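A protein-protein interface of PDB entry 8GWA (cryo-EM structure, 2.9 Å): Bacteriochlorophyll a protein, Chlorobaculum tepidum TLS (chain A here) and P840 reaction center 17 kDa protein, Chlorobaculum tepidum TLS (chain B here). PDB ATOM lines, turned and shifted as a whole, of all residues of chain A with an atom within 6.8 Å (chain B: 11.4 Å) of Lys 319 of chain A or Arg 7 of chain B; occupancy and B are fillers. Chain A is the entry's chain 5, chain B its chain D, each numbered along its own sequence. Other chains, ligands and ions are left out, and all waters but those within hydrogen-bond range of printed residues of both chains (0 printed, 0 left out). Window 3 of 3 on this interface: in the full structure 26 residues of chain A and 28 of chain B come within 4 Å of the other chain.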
ATOM      1  N   LEU A  20     -29.326 -19.997  11.342  1.00  0.00           N
ATOM      2  CA  LEU A  20     -30.144 -18.982  11.987  1.00  0.00           C
ATOM      3  C   LEU A  20     -29.798 -18.850  13.465  1.00  0.00           C
ATOM      4  O   LEU A  20     -29.087 -19.672  14.047  1.00  0.00           O
ATOM      5  CB  LEU A  20     -31.628 -19.313  11.816  1.00  0.00           C
ATOM      6  CG  LEU A  20     -32.089 -19.509  10.375  1.00  0.00           C
ATOM      7  CD1 LEU A  20     -33.569 -19.807  10.332  1.00  0.00           C
ATOM      8  CD2 LEU A  20     -31.783 -18.264   9.574  1.00  0.00           C
ATOM      9  N   GLY A  22     -31.728 -17.815  17.363  1.00  0.00           N
ATOM     10  CA  GLY A  22     -33.019 -18.015  17.977  1.00  0.00           C
ATOM     11  C   GLY A  22     -33.482 -16.854  18.838  1.00  0.00           C
ATOM     12  O   GLY A  22     -32.887 -15.775  18.869  1.00  0.00           O
ATOM     13  N   VAL A 316     -29.570 -24.610   8.937  1.00  0.00           N
ATOM     14  CA  VAL A 316     -29.303 -25.030  10.306  1.00  0.00           C
ATOM     15  C   VAL A 316     -30.113 -24.151  11.246  1.00  0.00           C
ATOM     16  O   VAL A 316     -29.762 -22.989  11.482  1.00  0.00           O
ATOM     17  CB  VAL A 316     -27.804 -24.956  10.636  1.00  0.00           C
ATOM     18  CG1 VAL A 316     -27.534 -25.593  11.984  1.00  0.00           C
ATOM     19  CG2 VAL A 316     -26.988 -25.631   9.549  1.00  0.00           C
ATOM     20  N   LEU A 317     -31.191 -24.699  11.781  1.00  0.00           N
ATOM     21  CA  LEU A 317     -32.007 -24.007  12.763  1.00  0.00           C
ATOM     22  C   LEU A 317     -31.294 -23.961  14.106  1.00  0.00           C
ATOM     23  O   LEU A 317     -30.371 -24.738  14.359  1.00  0.00           O
ATOM     24  CB  LEU A 317     -33.355 -24.709  12.910  1.00  0.00           C
ATOM     25  CG  LEU A 317     -34.297 -24.662  11.707  1.00  0.00           C
ATOM     26  CD1 LEU A 317     -35.710 -25.036  12.117  1.00  0.00           C
ATOM     27  CD2 LEU A 317     -34.277 -23.292  11.061  1.00  0.00           C
ATOM     28  N   PRO A 318     -31.675 -23.038  14.983  1.00  0.00           N
ATOM     29  CA  PRO A 318     -31.160 -23.073  16.355  1.00  0.00           C
ATOM     30  C   PRO A 318     -31.828 -24.172  17.169  1.00  0.00           C
ATOM     31  O   PRO A 318     -32.802 -24.797  16.746  1.00  0.00           O
ATOM     32  CB  PRO A 318     -31.496 -21.680  16.906  1.00  0.00           C
ATOM     33  CG  PRO A 318     -31.887 -20.858  15.705  1.00  0.00           C
ATOM     34  CD  PRO A 318     -32.457 -21.821  14.723  1.00  0.00           C
ATOM     35  N   LYS A 319     -31.271 -24.411  18.354  1.00  0.00           N
ATOM     36  CA  LYS A 319     -31.737 -25.508  19.194  1.00  0.00           C
ATOM     37  C   LYS A 319     -33.184 -25.303  19.623  1.00  0.00           C
ATOM     38  O   LYS A 319     -33.602 -24.194  19.967  1.00  0.00           O
ATOM     39  CB  LYS A 319     -30.842 -25.658  20.424  1.00  0.00           C
ATOM     40  CG  LYS A 319     -29.540 -26.399  20.167  1.00  0.00           C
ATOM     41  CD  LYS A 319     -28.524 -25.569  19.414  1.00  0.00           C
ATOM     42  CE  LYS A 319     -27.240 -26.345  19.238  1.00  0.00           C
ATOM     43  NZ  LYS A 319     -26.262 -25.628  18.384  1.00  0.00           N
ATOM     44  N   GLY A 320     -33.949 -26.395  19.604  1.00  0.00           N
ATOM     45  CA  GLY A 320     -35.354 -26.372  19.939  1.00  0.00           C
ATOM     46  C   GLY A 320     -36.269 -25.959  18.809  1.00  0.00           C
ATOM     47  O   GLY A 320     -37.488 -26.135  18.923  1.00  0.00           O
ATOM     48  N   TYR A 321     -35.716 -25.458  17.709  1.00  0.00           N
ATOM     49  CA  TYR A 321     -36.491 -24.919  16.598  1.00  0.00           C
ATOM     50  C   TYR A 321     -36.837 -26.026  15.611  1.00  0.00           C
ATOM     51  O   TYR A 321     -35.951 -26.589  14.960  1.00  0.00           O
ATOM     52  CB  TYR A 321     -35.696 -23.802  15.922  1.00  0.00           C
ATOM     53  CG  TYR A 321     -35.946 -22.443  16.526  1.00  0.00           C
ATOM     54  CD1 TYR A 321     -37.229 -21.940  16.635  1.00  0.00           C
ATOM     55  CD2 TYR A 321     -34.916 -21.720  17.092  1.00  0.00           C
ATOM     56  CE1 TYR A 321     -37.467 -20.709  17.211  1.00  0.00           C
ATOM     57  CE2 TYR A 321     -35.144 -20.500  17.678  1.00  0.00           C
ATOM     58  CZ  TYR A 321     -36.421 -19.996  17.737  1.00  0.00           C
ATOM     59  OH  TYR A 321     -36.647 -18.773  18.324  1.00  0.00           O
ATOM     60  N   LYS A 322     -38.124 -26.336  15.512  1.00  0.00           N
ATOM     61  CA  LYS A 322     -38.626 -27.304  14.555  1.00  0.00           C
ATOM     62  C   LYS A 322     -39.041 -26.595  13.267  1.00  0.00           C
ATOM     63  O   LYS A 322     -38.903 -25.380  13.124  1.00  0.00           O
ATOM     64  CB  LYS A 322     -39.798 -28.083  15.149  1.00  0.00           C
ATOM     65  CG  LYS A 322     -39.381 -29.281  15.988  1.00  0.00           C
ATOM     66  CD  LYS A 322     -39.049 -28.872  17.412  1.00  0.00           C
ATOM     67  CE  LYS A 322     -40.299 -28.526  18.196  1.00  0.00           C
ATOM     68  NZ  LYS A 322     -39.984 -28.155  19.602  1.00  0.00           N
ATOM     69  N   ASN A 334     -30.765 -33.687  10.150  1.00  0.00           N
ATOM     70  CA  ASN A 334     -29.923 -34.125  11.255  1.00  0.00           C
ATOM     71  C   ASN A 334     -30.278 -33.371  12.530  1.00  0.00           C
ATOM     72  O   ASN A 334     -29.385 -32.988  13.292  1.00  0.00           O
ATOM     73  CB  ASN A 334     -28.443 -33.932  10.919  1.00  0.00           C
ATOM     74  CG  ASN A 334     -27.548 -34.896  11.669  1.00  0.00           C
ATOM     75  OD1 ASN A 334     -27.907 -35.393  12.736  1.00  0.00           O
ATOM     76  ND2 ASN A 334     -26.371 -35.164  11.116  1.00  0.00           N
ATOM     77  N   LEU A 335     -31.576 -33.156  12.763  1.00  0.00           N
ATOM     78  CA  LEU A 335     -32.057 -32.483  13.966  1.00  0.00           C
ATOM     79  C   LEU A 335     -31.427 -31.101  14.076  1.00  0.00           C
ATOM     80  O   LEU A 335     -30.554 -30.892  14.923  1.00  0.00           O
ATOM     81  CB  LEU A 335     -31.780 -33.329  15.216  1.00  0.00           C
ATOM     82  CG  LEU A 335     -32.457 -32.959  16.545  1.00  0.00           C
ATOM     83  CD1 LEU A 335     -32.731 -34.229  17.297  1.00  0.00           C
ATOM     84  CD2 LEU A 335     -31.627 -32.042  17.429  1.00  0.00           C
ATOM     85  N   GLU A 336     -31.835 -30.195  13.171  1.00  0.00           N
ATOM     86  CA  GLU A 336     -31.350 -28.828  12.952  1.00  0.00           C
ATOM     87  C   GLU A 336     -30.842 -28.676  11.529  1.00  0.00           C
ATOM     88  O   GLU A 336     -31.322 -27.822  10.778  1.00  0.00           O
ATOM     89  CB  GLU A 336     -30.224 -28.409  13.895  1.00  0.00           C
ATOM     90  CG  GLU A 336     -30.682 -27.714  15.142  1.00  0.00           C
ATOM     91  CD  GLU A 336     -29.519 -27.179  15.934  1.00  0.00           C
ATOM     92  OE1 GLU A 336     -28.372 -27.596  15.667  1.00  0.00           O
ATOM     93  OE2 GLU A 336     -29.748 -26.320  16.802  1.00  0.00           O
ATOM     94  N   GLN A 366     -40.057 -22.903  17.281  1.00  0.00           N
ATOM     95  CA  GLN A 366     -39.758 -23.855  18.344  1.00  0.00           C
ATOM     96  C   GLN A 366     -41.015 -24.184  19.130  1.00  0.00           C
ATOM     97  O   GLN A 366     -42.031 -24.570  18.554  1.00  0.00           O
ATOM     98  CB  GLN A 366     -38.655 -23.314  19.270  1.00  0.00           C
ATOM     99  CG  GLN A 366     -38.956 -22.011  19.999  1.00  0.00           C
ATOM    100  CD  GLN A 366     -39.444 -22.225  21.414  1.00  0.00           C
ATOM    101  OE1 GLN A 366     -39.102 -23.218  22.056  1.00  0.00           O
ATOM    102  NE2 GLN A 366     -40.242 -21.290  21.914  1.00  0.00           N
ATOM    103  N   MET B   1     -21.253 -22.174  28.015  1.00  0.00           N
ATOM    104  CA  MET B   1     -20.557 -23.427  27.765  1.00  0.00           C
ATOM    105  C   MET B   1     -19.528 -23.201  26.661  1.00  0.00           C
ATOM    106  O   MET B   1     -19.750 -22.389  25.764  1.00  0.00           O
ATOM    107  CB  MET B   1     -21.554 -24.527  27.389  1.00  0.00           C
ATOM    108  CG  MET B   1     -20.941 -25.888  27.120  1.00  0.00           C
ATOM    109  SD  MET B   1     -22.083 -27.210  27.566  1.00  0.00           S
ATOM    110  CE  MET B   1     -21.119 -28.655  27.146  1.00  0.00           C
ATOM    111  N   GLN B   2     -18.404 -23.908  26.737  1.00  0.00           N
ATOM    112  CA  GLN B   2     -17.311 -23.666  25.807  1.00  0.00           C
ATOM    113  C   GLN B   2     -17.756 -23.959  24.375  1.00  0.00           C
ATOM    114  O   GLN B   2     -18.543 -24.885  24.146  1.00  0.00           O
ATOM    115  CB  GLN B   2     -16.098 -24.528  26.163  1.00  0.00           C
ATOM    116  CG  GLN B   2     -15.410 -24.130  27.456  1.00  0.00           C
ATOM    117  CD  GLN B   2     -14.219 -25.013  27.775  1.00  0.00           C
ATOM    118  OE1 GLN B   2     -13.932 -25.970  27.059  1.00  0.00           O
ATOM    119  NE2 GLN B   2     -13.519 -24.693  28.857  1.00  0.00           N
ATOM    120  N   PRO B   3     -17.289 -23.183  23.393  1.00  0.00           N
ATOM    121  CA  PRO B   3     -17.696 -23.445  22.003  1.00  0.00           C
ATOM    122  C   PRO B   3     -17.276 -24.813  21.498  1.00  0.00           C
ATOM    123  O   PRO B   3     -18.011 -25.421  20.711  1.00  0.00           O
ATOM    124  CB  PRO B   3     -17.020 -22.319  21.207  1.00  0.00           C
ATOM    125  CG  PRO B   3     -15.968 -21.761  22.090  1.00  0.00           C
ATOM    126  CD  PRO B   3     -16.275 -22.120  23.508  1.00  0.00           C
ATOM    127  N   GLN B   4     -16.128 -25.325  21.935  1.00  0.00           N
ATOM    128  CA  GLN B   4     -15.635 -26.614  21.469  1.00  0.00           C
ATOM    129  C   GLN B   4     -16.299 -27.789  22.170  1.00  0.00           C
ATOM    130  O   GLN B   4     -16.054 -28.937  21.788  1.00  0.00           O
ATOM    131  CB  GLN B   4     -14.117 -26.702  21.653  1.00  0.00           C
ATOM    132  CG  GLN B   4     -13.659 -26.782  23.098  1.00  0.00           C
ATOM    133  CD  GLN B   4     -13.450 -25.416  23.720  1.00  0.00           C
ATOM    134  OE1 GLN B   4     -13.906 -24.403  23.191  1.00  0.00           O
ATOM    135  NE2 GLN B   4     -12.756 -25.382  24.851  1.00  0.00           N
ATOM    136  N   LEU B   5     -17.127 -27.535  23.180  1.00  0.00           N
ATOM    137  CA  LEU B   5     -17.857 -28.584  23.875  1.00  0.00           C
ATOM    138  C   LEU B   5     -19.348 -28.540  23.577  1.00  0.00           C
ATOM    139  O   LEU B   5     -20.119 -29.269  24.208  1.00  0.00           O
ATOM    140  CB  LEU B   5     -17.620 -28.480  25.383  1.00  0.00           C
ATOM    141  CG  LEU B   5     -16.403 -29.229  25.925  1.00  0.00           C
ATOM    142  CD1 LEU B   5     -16.136 -28.835  27.365  1.00  0.00           C
ATOM    143  CD2 LEU B   5     -16.596 -30.729  25.807  1.00  0.00           C
ATOM    144  N   SER B   6     -19.768 -27.713  22.627  1.00  0.00           N
ATOM    145  CA  SER B   6     -21.173 -27.535  22.301  1.00  0.00           C
ATOM    146  C   SER B   6     -21.445 -28.008  20.880  1.00  0.00           C
ATOM    147  O   SER B   6     -20.524 -28.237  20.090  1.00  0.00           O
ATOM    148  CB  SER B   6     -21.596 -26.067  22.454  1.00  0.00           C
ATOM    149  OG  SER B   6     -20.748 -25.214  21.706  1.00  0.00           O
ATOM    150  N   ARG B   7     -22.727 -28.164  20.572  1.00  0.00           N
ATOM    151  CA  ARG B   7     -23.128 -28.537  19.226  1.00  0.00           C
ATOM    152  C   ARG B   7     -22.661 -27.459  18.247  1.00  0.00           C
ATOM    153  O   ARG B   7     -22.753 -26.266  18.556  1.00  0.00           O
ATOM    154  CB  ARG B   7     -24.646 -28.718  19.165  1.00  0.00           C
ATOM    155  CG  ARG B   7     -25.168 -29.415  17.921  1.00  0.00           C
ATOM    156  CD  ARG B   7     -24.879 -30.907  17.983  1.00  0.00           C
ATOM    157  NE  ARG B   7     -25.884 -31.642  18.741  1.00  0.00           N
ATOM    158  CZ  ARG B   7     -26.944 -32.229  18.205  1.00  0.00           C
ATOM    159  NH1 ARG B   7     -27.174 -32.188  16.904  1.00  0.00           N
ATOM    160  NH2 ARG B   7     -27.795 -32.879  18.995  1.00  0.00           N
ATOM    161  N   PRO B   8     -22.140 -27.845  17.067  1.00  0.00           N
ATOM    162  CA  PRO B   8     -21.391 -26.899  16.223  1.00  0.00           C
ATOM    163  C   PRO B   8     -22.040 -25.544  15.978  1.00  0.00           C
ATOM    164  O   PRO B   8     -21.439 -24.512  16.293  1.00  0.00           O
ATOM    165  CB  PRO B   8     -21.242 -27.672  14.909  1.00  0.00           C
ATOM    166  CG  PRO B   8     -21.201 -29.099  15.325  1.00  0.00           C
ATOM    167  CD  PRO B   8     -21.979 -29.235  16.607  1.00  0.00           C
ATOM    168  N   GLN B   9     -23.252 -25.517  15.427  1.00  0.00           N
ATOM    169  CA  GLN B   9     -23.907 -24.249  15.104  1.00  0.00           C
ATOM    170  C   GLN B   9     -24.746 -23.801  16.296  1.00  0.00           C
ATOM    171  O   GLN B   9     -25.974 -23.908  16.319  1.00  0.00           O
ATOM    172  CB  GLN B   9     -24.744 -24.377  13.838  1.00  0.00           C
ATOM    173  CG  GLN B   9     -23.953 -24.215  12.551  1.00  0.00           C
ATOM    174  CD  GLN B   9     -23.389 -25.517  12.041  1.00  0.00           C
ATOM    175  OE1 GLN B   9     -23.757 -26.592  12.510  1.00  0.00           O
ATOM    176  NE2 GLN B   9     -22.494 -25.428  11.066  1.00  0.00           N
ATOM    177  N   THR B  10     -24.054 -23.281  17.308  1.00  0.00           N
ATOM    178  CA  THR B  10     -24.685 -22.715  18.492  1.00  0.00           C
ATOM    179  C   THR B  10     -24.277 -21.254  18.602  1.00  0.00           C
ATOM    180  O   THR B  10     -23.082 -20.943  18.651  1.00  0.00           O
ATOM    181  CB  THR B  10     -24.287 -23.476  19.758  1.00  0.00           C
ATOM    182  OG1 THR B  10     -24.336 -24.884  19.502  1.00  0.00           O
ATOM    183  CG2 THR B  10     -25.245 -23.154  20.890  1.00  0.00           C
ATOM    184  N   ALA B  11     -25.262 -20.366  18.637  1.00  0.00           N
ATOM    185  CA  ALA B  11     -25.008 -18.943  18.778  1.00  0.00           C
ATOM    186  C   ALA B  11     -24.900 -18.565  20.252  1.00  0.00           C
ATOM    187  O   ALA B  11     -25.276 -19.325  21.147  1.00  0.00           O
ATOM    188  CB  ALA B  11     -26.110 -18.133  18.096  1.00  0.00           C
ATOM    189  N   SER B  12     -24.367 -17.366  20.500  1.00  0.00           N
ATOM    190  CA  SER B  12     -24.281 -16.864  21.866  1.00  0.00           C
ATOM    191  C   SER B  12     -25.654 -16.705  22.502  1.00  0.00           C
ATOM    192  O   SER B  12     -25.758 -16.699  23.734  1.00  0.00           O
ATOM    193  CB  SER B  12     -23.534 -15.530  21.889  1.00  0.00           C
ATOM    194  OG  SER B  12     -24.222 -14.547  21.135  1.00  0.00           O
ATOM    195  N   ASN B  13     -26.704 -16.569  21.691  1.00  0.00           N
ATOM    196  CA  ASN B  13     -28.060 -16.545  22.228  1.00  0.00           C
ATOM    197  C   ASN B  13     -28.398 -17.871  22.898  1.00  0.00           C
ATOM    198  O   ASN B  13     -29.146 -17.908  23.883  1.00  0.00           O
ATOM    199  CB  ASN B  13     -29.048 -16.224  21.105  1.00  0.00           C
ATOM    200  CG  ASN B  13     -30.459 -15.969  21.607  1.00  0.00           C
ATOM    201  OD1 ASN B  13     -30.739 -16.051  22.802  1.00  0.00           O
ATOM    202  ND2 ASN B  13     -31.356 -15.641  20.686  1.00  0.00           N
ATOM    203  N   GLN B  14     -27.839 -18.971  22.393  1.00  0.00           N
ATOM    204  CA  GLN B  14     -28.083 -20.287  22.965  1.00  0.00           C
ATOM    205  C   GLN B  14     -26.872 -20.844  23.700  1.00  0.00           C
ATOM    206  O   GLN B  14     -26.994 -21.851  24.403  1.00  0.00           O
ATOM    207  CB  GLN B  14     -28.524 -21.265  21.873  1.00  0.00           C
ATOM    208  CG  GLN B  14     -29.858 -20.907  21.237  1.00  0.00           C
ATOM    209  CD  GLN B  14     -30.396 -22.008  20.348  1.00  0.00           C
ATOM    210  OE1 GLN B  14     -29.675 -22.559  19.517  1.00  0.00           O
ATOM    211  NE2 GLN B  14     -31.672 -22.335  20.518  1.00  0.00           N
ATOM    212  N   VAL B  15     -25.695 -20.245  23.534  1.00  0.00           N
ATOM    213  CA  VAL B  15     -24.582 -20.566  24.416  1.00  0.00           C
ATOM    214  C   VAL B  15     -24.811 -19.891  25.762  1.00  0.00           C
ATOM    215  O   VAL B  15     -24.980 -18.666  25.837  1.00  0.00           O
ATOM    216  CB  VAL B  15     -23.249 -20.129  23.791  1.00  0.00           C
ATOM    217  CG1 VAL B  15     -22.149 -20.133  24.836  1.00  0.00           C
ATOM    218  CG2 VAL B  15     -22.884 -21.040  22.633  1.00  0.00           C
ATOM    219  N   ARG B  16     -24.825 -20.681  26.831  1.00  0.00           N
ATOM    220  CA  ARG B  16     -25.042 -20.154  28.171  1.00  0.00           C
ATOM    221  C   ARG B  16     -23.718 -19.990  28.907  1.00  0.00           C
ATOM    222  O   ARG B  16     -22.862 -20.880  28.884  1.00  0.00           O
ATOM    223  CB  ARG B  16     -25.990 -21.042  28.989  1.00  0.00           C
ATOM    224  CG  ARG B  16     -25.421 -22.389  29.416  1.00  0.00           C
ATOM    225  CD  ARG B  16     -26.478 -23.297  30.032  1.00  0.00           C
ATOM    226  NE  ARG B  16     -27.356 -22.580  30.951  1.00  0.00           N
ATOM    227  CZ  ARG B  16     -28.566 -22.987  31.308  1.00  0.00           C
ATOM    228  NH1 ARG B  16     -29.087 -24.107  30.834  1.00  0.00           N
ATOM    229  NH2 ARG B  16     -29.269 -22.257  32.168  1.00  0.00           N
ATOM    230  N   ALA B  27     -34.037 -25.201  34.591  1.00  0.00           N
ATOM    231  CA  ALA B  27     -33.151 -25.788  33.594  1.00  0.00           C
ATOM    232  C   ALA B  27     -33.646 -25.569  32.171  1.00  0.00           C
ATOM    233  O   ALA B  27     -32.857 -25.695  31.228  1.00  0.00           O
ATOM    234  CB  ALA B  27     -32.983 -27.286  33.855  1.00  0.00           C
ATOM    235  N   VAL B  28     -34.930 -25.254  31.997  1.00  0.00           N
ATOM    236  CA  VAL B  28     -35.469 -25.030  30.661  1.00  0.00           C
ATOM    237  C   VAL B  28     -34.887 -23.761  30.052  1.00  0.00           C
ATOM    238  O   VAL B  28     -34.610 -23.705  28.848  1.00  0.00           O
ATOM    239  CB  VAL B  28     -37.007 -24.980  30.716  1.00  0.00           C
ATOM    240  CG1 VAL B  28     -37.584 -24.739  29.332  1.00  0.00           C
ATOM    241  CG2 VAL B  28     -37.559 -26.262  31.311  1.00  0.00           C
ATOM    242  N   HIS B  29     -34.680 -22.733  30.868  1.00  0.00           N
ATOM    243  CA  HIS B  29     -34.262 -21.422  30.390  1.00  0.00           C
ATOM    244  C   HIS B  29     -32.762 -21.248  30.577  1.00  0.00           C
ATOM    245  O   HIS B  29     -32.264 -21.259  31.707  1.00  0.00           O
ATOM    246  CB  HIS B  29     -35.022 -20.315  31.117  1.00  0.00           C
ATOM    247  CG  HIS B  29     -36.488 -20.571  31.224  1.00  0.00           C
ATOM    248  ND1 HIS B  29     -37.210 -21.159  30.210  1.00  0.00           N
ATOM    249  CD2 HIS B  29     -37.370 -20.323  32.221  1.00  0.00           C
ATOM    250  CE1 HIS B  29     -38.475 -21.263  30.575  1.00  0.00           C
ATOM    251  NE2 HIS B  29     -38.599 -20.762  31.791  1.00  0.00           N
ATOM    252  N   LYS B  30     -32.050 -21.088  29.461  1.00  0.00           N
ATOM    253  CA  LYS B  30     -30.636 -20.748  29.523  1.00  0.00           C
ATOM    254  C   LYS B  30     -30.433 -19.377  30.154  1.00  0.00           C
ATOM    255  O   LYS B  30     -29.509 -19.179  30.951  1.00  0.00           O
ATOM    256  CB  LYS B  30     -30.041 -20.795  28.120  1.00  0.00           C
ATOM    257  CG  LYS B  30     -30.008 -22.190  27.535  1.00  0.00           C
ATOM    258  CD  LYS B  30     -29.368 -22.182  26.172  1.00  0.00           C
ATOM    259  CE  LYS B  30     -29.396 -23.554  25.537  1.00  0.00           C
ATOM    260  NZ  LYS B  30     -28.518 -24.502  26.273  1.00  0.00           N
ATOM    261  N   GLU B  76     -34.472 -12.833  28.994  1.00  0.00           N
ATOM    262  CA  GLU B  76     -35.368 -12.865  27.847  1.00  0.00           C
ATOM    263  C   GLU B  76     -36.772 -12.482  28.288  1.00  0.00           C
ATOM    264  O   GLU B  76     -37.193 -12.808  29.401  1.00  0.00           O
ATOM    265  CB  GLU B  76     -35.379 -14.246  27.187  1.00  0.00           C
ATOM    266  CG  GLU B  76     -34.063 -14.619  26.528  1.00  0.00           C
ATOM    267  CD  GLU B  76     -34.096 -15.996  25.901  1.00  0.00           C
ATOM    268  OE1 GLU B  76     -35.103 -16.709  26.086  1.00  0.00           O
ATOM    269  OE2 GLU B  76     -33.113 -16.366  25.225  1.00  0.00           O
ATOM    270  N   TYR B  78     -40.949 -12.259  27.145  1.00  0.00           N
ATOM    271  CA  TYR B  78     -42.005 -12.771  26.284  1.00  0.00           C
ATOM    272  C   TYR B  78     -43.334 -12.153  26.700  1.00  0.00           C
ATOM    273  O   TYR B  78     -43.461 -11.560  27.774  1.00  0.00           O
ATOM    274  CB  TYR B  78     -42.068 -14.304  26.328  1.00  0.00           C
ATOM    275  CG  TYR B  78     -40.796 -14.962  25.846  1.00  0.00           C
ATOM    276  CD1 TYR B  78     -39.700 -15.099  26.687  1.00  0.00           C
ATOM    277  CD2 TYR B  78     -40.678 -15.417  24.541  1.00  0.00           C
ATOM    278  CE1 TYR B  78     -38.532 -15.688  26.248  1.00  0.00           C
ATOM    279  CE2 TYR B  78     -39.513 -16.008  24.093  1.00  0.00           C
ATOM    280  CZ  TYR B  78     -38.444 -16.141  24.951  1.00  0.00           C
ATOM    281  OH  TYR B  78     -37.282 -16.729  24.509  1.00  0.00           O
ATOM    282  N   GLU B 116     -45.986 -17.763  22.894  1.00  0.00           N
ATOM    283  CA  GLU B 116     -45.206 -16.630  23.370  1.00  0.00           C
ATOM    284  C   GLU B 116     -44.475 -15.986  22.201  1.00  0.00           C
ATOM    285  O   GLU B 116     -44.055 -16.671  21.262  1.00  0.00           O
ATOM    286  CB  GLU B 116     -44.197 -17.044  24.447  1.00  0.00           C
ATOM    287  CG  GLU B 116     -43.055 -17.905  23.939  1.00  0.00           C
ATOM    288  CD  GLU B 116     -42.290 -18.594  25.050  1.00  0.00           C
ATOM    289  OE1 GLU B 116     -42.900 -18.936  26.083  1.00  0.00           O
ATOM    290  OE2 GLU B 116     -41.064 -18.781  24.890  1.00  0.00           O
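Of chain B, only Arg 7 (3.5 Å), Gln 9 (2.7 Å), Thr 10 (2.3 Å) and Gln 14 (2.7 Å) come within 4 Å of Lys 319 of chain A.
Of chain A, only Lys 319 comes within 4 Å of Arg 7 of chain B.
Pro 318 of chain A touches one residue of chain B.
Gly 320 of chain A touches none of the printed residues of chain B.
No residue of chain B comes within 4 Å of Tyr 321 of chain A.
No residue of chain B comes within 4 Å of Leu 335 of chain A.
Of the printed residues of chain A, Glu 116 of chain B touches Gln 366.
Of the printed residues of chain A, Thr 10 of chain B touches Lys 319.
Of the printed residues of chain A, Asn 13 of chain B touches Gly 22.
Leu 20 of chain A touches none of the printed residues of chain B.
The nearest residue of chain A that does not touch Arg 7 of chain B is Leu 335 of chain A (4.1 Å).
The nearest printed residue of chain A that does not touch Thr 10 of chain B is Glu 336 of chain A (6.2 Å).
N of Leu 20 of chain A sits at hydrogen-bond distance from O of Val 316 of chain A.
The side-chain amino group of Lys 319 of chain A lies within salt-bridge range of the side-chain carboxylate of Glu 336 of chain A.
The side-chain amide oxygen (OD1) of Asn 13 of chain B sits close to the side-chain carboxylate (OE2) of Glu 76 of chain B (3.4 Å).
Gln 9 of chain B touches Val 316 of chain A.
CB of Pro 318 of chain A touches OE1 of Gln 14 of chain B, at 3.3 Å.
CB of Arg 7 of chain B touches CE of Lys 319 of chain A, 3.5 Å away.
Gln 366 of chain A touches Glu 116 of chain B (NE2 to OE2, 3.98 Å).
Hydrophobic or aromatic side chains of chain A within 4 Å of the printed part of chain B: Val 316 and Pro 318.
Along chain A the printed residues that touch a printed residue of chain B span positions 22 to 366.
Of the 23 printed residues of chain B, 6 touch a printed residue of chain A.
Among the printed residues, 8 pairs touch across the chains.
Among the printed residues, no Asp or Glu carboxylate lies within 4 Å of a Lys or Arg side-chain nitrogen of the other chain.
The backbone carbonyl oxygen (O) of Gln 9 of chain B is in hydrogen-bond range of the side-chain amino group (NZ) of Lys 319 of chain A (2.7 Å).
The backbone NH of Lys 319 of chain A lies within hydrogen-bond range of the side-chain amide oxygen of Gln 14 of chain B (2.7 Å).
O of Gly 22 of chain A lies close to ND2 of Asn 13 of chain B (2.4 Å).
The side-chain amino group of Lys 319 of chain A sits close to the side-chain hydroxyl of Thr 10 of chain B (2.3 Å).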
